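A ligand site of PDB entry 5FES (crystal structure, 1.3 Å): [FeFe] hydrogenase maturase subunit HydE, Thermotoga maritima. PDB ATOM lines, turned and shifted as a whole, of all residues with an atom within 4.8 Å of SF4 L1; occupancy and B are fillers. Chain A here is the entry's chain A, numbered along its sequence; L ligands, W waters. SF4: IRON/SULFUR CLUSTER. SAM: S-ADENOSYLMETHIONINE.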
ATOM      1  N   CYS A  73       6.762  -5.824 -21.206  1.00  0.00           N
ATOM      2  CA  CYS A  73       5.566  -6.306 -21.842  1.00  0.00           C
ATOM      3  C   CYS A  73       5.848  -6.892 -23.235  1.00  0.00           C
ATOM      4  O   CYS A  73       6.595  -6.320 -24.028  1.00  0.00           O
ATOM      5  CB  CYS A  73       4.471  -5.235 -21.978  1.00  0.00           C
ATOM      6  SG  CYS A  73       2.856  -5.972 -22.326  1.00  0.00           S
ATOM      7  N   LYS A  75       3.213  -7.430 -25.347  1.00  0.00           N
ATOM      8  CA  LYS A  75       2.192  -6.911 -26.217  1.00  0.00           C
ATOM      9  C   LYS A  75       2.517  -5.497 -26.654  1.00  0.00           C
ATOM     10  O   LYS A  75       3.455  -4.844 -26.192  1.00  0.00           O
ATOM     11  CB  LYS A  75       0.818  -6.956 -25.558  1.00  0.00           C
ATOM     12  CG  LYS A  75       0.194  -8.379 -25.580  1.00  0.00           C
ATOM     13  CD  LYS A  75      -1.199  -8.362 -25.077  1.00  0.00           C
ATOM     14  CE  LYS A  75      -1.996  -9.651 -25.379  1.00  0.00           C
ATOM     15  NZ  LYS A  75      -1.337 -10.892 -24.983  1.00  0.00           N
ATOM     16  N   ASN A  76       1.759  -5.027 -27.663  1.00  0.00           N
ATOM     17  CA  ASN A  76       2.057  -3.791 -28.386  1.00  0.00           C
ATOM     18  C   ASN A  76       0.837  -2.868 -28.477  1.00  0.00           C
ATOM     19  O   ASN A  76       0.656  -2.186 -29.477  1.00  0.00           O
ATOM     20  CB  ASN A  76       2.610  -4.097 -29.787  1.00  0.00           C
ATOM     21  CG  ASN A  76       3.623  -3.101 -30.265  1.00  0.00           C
ATOM     22  OD1 ASN A  76       4.303  -2.405 -29.524  1.00  0.00           O
ATOM     23  ND2 ASN A  76       3.796  -3.096 -31.623  1.00  0.00           N
ATOM     24  N   CYS A  77       0.016  -2.838 -27.453  1.00  0.00           N
ATOM     25  CA  CYS A  77      -1.179  -2.010 -27.489  1.00  0.00           C
ATOM     26  C   CYS A  77      -0.860  -0.581 -27.863  1.00  0.00           C
ATOM     27  O   CYS A  77       0.100   0.005 -27.357  1.00  0.00           O
ATOM     28  CB  CYS A  77      -1.890  -2.099 -26.077  1.00  0.00           C
ATOM     29  SG  CYS A  77      -2.201  -3.734 -25.470  1.00  0.00           S
ATOM     30  N   TYR A  79      -2.110   2.301 -27.357  1.00  0.00           N
ATOM     31  CA  TYR A  79      -2.285   3.383 -26.371  1.00  0.00           C
ATOM     32  C   TYR A  79      -1.244   3.444 -25.268  1.00  0.00           C
ATOM     33  O   TYR A  79      -1.102   4.455 -24.564  1.00  0.00           O
ATOM     34  CB  TYR A  79      -3.651   3.316 -25.741  1.00  0.00           C
ATOM     35  CG  TYR A  79      -4.126   1.964 -25.346  1.00  0.00           C
ATOM     36  CD1 TYR A  79      -3.686   1.388 -24.166  1.00  0.00           C
ATOM     37  CD2 TYR A  79      -4.947   1.179 -26.105  1.00  0.00           C
ATOM     38  CE1 TYR A  79      -4.077   0.130 -23.756  1.00  0.00           C
ATOM     39  CE2 TYR A  79      -5.346  -0.101 -25.771  1.00  0.00           C
ATOM     40  CZ  TYR A  79      -4.888  -0.628 -24.557  1.00  0.00           C
ATOM     41  OH  TYR A  79      -5.333  -1.896 -24.258  1.00  0.00           O
ATOM     42  N   CYS A  80      -0.517   2.309 -25.054  1.00  0.00           N
ATOM     43  CA  CYS A  80       0.192   2.123 -23.797  1.00  0.00           C
ATOM     44  C   CYS A  80       1.697   2.402 -23.886  1.00  0.00           C
ATOM     45  O   CYS A  80       2.371   1.830 -24.783  1.00  0.00           O
ATOM     46  CB  CYS A  80       0.034   0.666 -23.379  1.00  0.00           C
ATOM     47  SG  CYS A  80       0.747   0.299 -21.724  1.00  0.00           S
ATOM     48  N   LEU A  82       3.977   1.195 -22.142  1.00  0.00           N
ATOM     49  CA  LEU A  82       4.743  -0.038 -21.886  1.00  0.00           C
ATOM     50  C   LEU A  82       4.788  -0.969 -23.128  1.00  0.00           C
ATOM     51  O   LEU A  82       5.456  -1.996 -23.083  1.00  0.00           O
ATOM     52  CB  LEU A  82       4.231  -0.828 -20.693  1.00  0.00           C
ATOM     53  CG  LEU A  82       4.071  -0.010 -19.404  1.00  0.00           C
ATOM     54  CD1 LEU A  82       3.820  -1.072 -18.255  1.00  0.00           C
ATOM     55  CD2 LEU A  82       5.152   0.905 -19.004  1.00  0.00           C
ATOM     56  N   ARG A  83       4.169  -0.563 -24.224  1.00  0.00           N
ATOM     57  CA  ARG A  83       4.116  -1.419 -25.415  1.00  0.00           C
ATOM     58  C   ARG A  83       5.554  -1.847 -25.790  1.00  0.00           C
ATOM     59  O   ARG A  83       6.490  -1.085 -25.688  1.00  0.00           O
ATOM     60  CB  ARG A  83       3.386  -0.701 -26.542  1.00  0.00           C
ATOM     61  CG  ARG A  83       4.096   0.517 -27.109  1.00  0.00           C
ATOM     62  CD  ARG A  83       3.183   1.388 -27.926  1.00  0.00           C
ATOM     63  NE  ARG A  83       2.476   0.662 -28.939  1.00  0.00           N
ATOM     64  CZ  ARG A  83       2.922   0.460 -30.216  1.00  0.00           C
ATOM     65  NH1 ARG A  83       4.036   1.054 -30.616  1.00  0.00           N
ATOM     66  NH2 ARG A  83       2.177  -0.254 -31.034  1.00  0.00           N
ATOM     67  N   SER A 118       1.482  -5.697 -13.612  1.00  0.00           N
ATOM     68  CA  SER A 118       2.658  -5.651 -14.450  1.00  0.00           C
ATOM     69  C   SER A 118       2.257  -5.550 -15.891  1.00  0.00           C
ATOM     70  O   SER A 118       1.109  -5.788 -16.269  1.00  0.00           O
ATOM     71  CB  SER A 118       3.547  -6.904 -14.223  1.00  0.00           C
ATOM     72  OG  SER A 118       2.852  -8.089 -14.568  1.00  0.00           O
ATOM     73  N   GLY A 119       3.277  -5.232 -16.737  1.00  0.00           N
ATOM     74  CA  GLY A 119       3.163  -5.629 -18.143  1.00  0.00           C
ATOM     75  C   GLY A 119       3.005  -7.126 -18.260  1.00  0.00           C
ATOM     76  O   GLY A 119       3.215  -7.900 -17.305  1.00  0.00           O
ATOM     77  N   GLU A 120       2.656  -7.595 -19.462  1.00  0.00           N
ATOM     78  CA  GLU A 120       2.643  -9.023 -19.714  1.00  0.00           C
ATOM     79  C   GLU A 120       4.087  -9.497 -19.864  1.00  0.00           C
ATOM     80  O   GLU A 120       4.617  -9.644 -21.009  1.00  0.00           O
ATOM     81  CB  GLU A 120       1.811  -9.378 -20.953  1.00  0.00           C
ATOM     82  CG  GLU A 120       0.315  -9.142 -20.758  1.00  0.00           C
ATOM     83  CD  GLU A 120      -0.518  -9.837 -21.792  1.00  0.00           C
ATOM     84  OE1 GLU A 120      -0.001 -10.590 -22.637  1.00  0.00           O
ATOM     85  OE2 GLU A 120      -1.777  -9.615 -21.773  1.00  0.00           O
ATOM     86  N   ARG A 182      -5.291  -3.226 -30.104  1.00  0.00           N
ATOM     87  CA  ARG A 182      -4.623  -4.299 -29.364  1.00  0.00           C
ATOM     88  C   ARG A 182      -4.318  -5.470 -30.365  1.00  0.00           C
ATOM     89  O   ARG A 182      -4.969  -6.487 -30.374  1.00  0.00           O
ATOM     90  CB  ARG A 182      -5.478  -4.798 -28.188  1.00  0.00           C
ATOM     91  CG  ARG A 182      -5.946  -3.619 -27.329  1.00  0.00           C
ATOM     92  CD  ARG A 182      -6.670  -4.039 -26.055  1.00  0.00           C
ATOM     93  NE  ARG A 182      -5.691  -4.694 -25.158  1.00  0.00           N
ATOM     94  CZ  ARG A 182      -5.617  -5.959 -24.865  1.00  0.00           C
ATOM     95  NH1 ARG A 182      -6.580  -6.784 -25.109  1.00  0.00           N
ATOM     96  NH2 ARG A 182      -4.513  -6.387 -24.216  1.00  0.00           N
HETATM   97 FE1  SF4 L   1       0.289  -1.940 -21.785  1.00  0.00          FE
HETATM   98 FE2  SF4 L   1       1.204  -4.428 -22.168  1.00  0.00          FE
HETATM   99 FE3  SF4 L   1      -1.081  -3.633 -23.410  1.00  0.00          FE
HETATM  100 FE4  SF4 L   1      -1.128  -4.113 -20.594  1.00  0.00          FE
HETATM  101  S1  SF4 L   1      -0.780  -5.624 -22.365  1.00  0.00           S
HETATM  102  S2  SF4 L   1      -1.991  -2.244 -21.776  1.00  0.00           S
HETATM  103  S3  SF4 L   1       1.058  -3.300 -20.173  1.00  0.00           S
HETATM  104  S4  SF4 L   1       1.066  -2.841 -23.778  1.00  0.00           S
HETATM  105  N   SAM L   2      -0.928  -5.588 -18.892  1.00  0.00           N
HETATM  106  CA  SAM L   2      -2.090  -5.753 -18.005  1.00  0.00           C
HETATM  107  C   SAM L   2      -3.290  -5.348 -18.837  1.00  0.00           C
HETATM  108  O   SAM L   2      -4.420  -5.708 -18.449  1.00  0.00           O
HETATM  109  OXT SAM L   2      -3.093  -4.709 -19.916  1.00  0.00           O
HETATM  110  CB  SAM L   2      -1.944  -4.878 -16.768  1.00  0.00           C
HETATM  111  CG  SAM L   2      -1.159  -3.507 -16.991  1.00  0.00           C
HETATM  112  SD  SAM L   2      -1.953  -2.280 -18.057  1.00  0.00           S
HETATM  113  CE  SAM L   2      -0.808  -0.986 -17.969  1.00  0.00           C
HETATM  114  C5' SAM L   2      -3.299  -1.700 -17.008  1.00  0.00           C
HETATM  115  C4' SAM L   2      -4.335  -0.762 -17.710  1.00  0.00           C
HETATM  116  O4' SAM L   2      -3.662   0.480 -18.056  1.00  0.00           O
HETATM  117  C3' SAM L   2      -4.959  -1.207 -18.985  1.00  0.00           C
HETATM  118  O3' SAM L   2      -6.019  -2.079 -18.666  1.00  0.00           O
HETATM  119  C2' SAM L   2      -5.389   0.145 -19.648  1.00  0.00           C
HETATM  120  O2' SAM L   2      -6.820   0.414 -19.497  1.00  0.00           O
HETATM  121  C1' SAM L   2      -4.607   1.231 -18.916  1.00  0.00           C
HETATM  122  N9  SAM L   2      -3.840   2.068 -19.782  1.00  0.00           N
HETATM  123  C8  SAM L   2      -2.826   1.682 -20.616  1.00  0.00           C
HETATM  124  N7  SAM L   2      -2.404   2.748 -21.336  1.00  0.00           N
HETATM  125  C5  SAM L   2      -3.212   3.819 -20.979  1.00  0.00           C
HETATM  126  C6  SAM L   2      -3.268   5.140 -21.403  1.00  0.00           C
HETATM  127  N6  SAM L   2      -2.464   5.638 -22.411  1.00  0.00           N
HETATM  128  N1  SAM L   2      -4.203   5.973 -20.902  1.00  0.00           N
HETATM  129  C2  SAM L   2      -4.920   5.478 -19.834  1.00  0.00           C
HETATM  130  N3  SAM L   2      -4.951   4.245 -19.409  1.00  0.00           N
HETATM  131  C4  SAM L   2      -4.074   3.392 -19.994  1.00  0.00           C
HETATM  132  O   HOH W   1      -3.247  -7.414 -21.221  1.00  0.00           O
HETATM  133  O   HOH W   2      -4.803  -3.734 -22.340  1.00  0.00           O
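An iron atom (FE4) of SF4 L1 is bound by an oxygen (OXT) of SAM L2, 2.2 Å away.
Water W2 lies within hydrogen-bond range of OH of Tyr 79 (2.7 Å), NE of Arg 182 (3.1 Å) and S2 of SF4 L1 (3.2 Å). Water W1 lies within hydrogen-bond range of the side-chain carboxylate (OE2) of Glu 120 (2.7 Å), a sulfur (S1) of SF4 L1 (3.3 Å), the guanidinium group (NH2) of Arg 182 (3.4 Å) and an oxygen (O) of SAM L2 (3.5 Å).
The backbone carbonyl oxygen (O) of Cys 77 is in hydrogen-bond range of the guanidinium group (NE) of Arg 83 (2.9 Å). OH of Tyr 79 lies within hydrogen-bond range of NE of Arg 182 (3.0 Å). NH2 of Arg 83 lies within hydrogen-bond range of O of Asn 76. The side-chain sulfur of Cys 73 lies close to the backbone NH of Glu 120, at 3.3 Å. NE of Arg 182 lies close to SG of Cys 77, at 3.6 Å. N of Lys 75 lies close to SG of Cys 73 (3.4 Å). SG of Cys 80 sits close to N of Leu 82 (3.4 Å). NZ of Lys 75 is in salt-bridge range of OE1 of Glu 120, 2.7 Å away.
The side-chain sulfur (SG) of Cys 77 is bound to an iron atom (FE3) of SF4 L1 (2.3 Å). O of Ser 118 lies close to N of SAM L2, 3.3 Å away. An iron atom (FE1) of SF4 L1 is bound by the side-chain sulfur of Cys 80 (2.3 Å). An iron atom (FE2) of SF4 L1 is bound by the side-chain sulfur of Cys 73 (2.3 Å). N6 of SAM L2 sits at hydrogen-bond distance from O of Tyr 79 (2.8 Å).
Lys 75 touches SF4 L1 (CB to S1, 3.8 Å). Tyr 79 touches SF4 L1 (CE1 to S2, 3.7 Å). Arg 83 touches SF4 L1. CA of Gly 119 touches S3 of SF4 L1, at 3.7 Å. Within 4 Å of SF4 L1: Cys 73, Lys 75, Cys 77, Tyr 79, Cys 80, Arg 83 and Gly 119. Along chain A the residues within 4 Å of SF4 L1 span positions 73 to 119.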
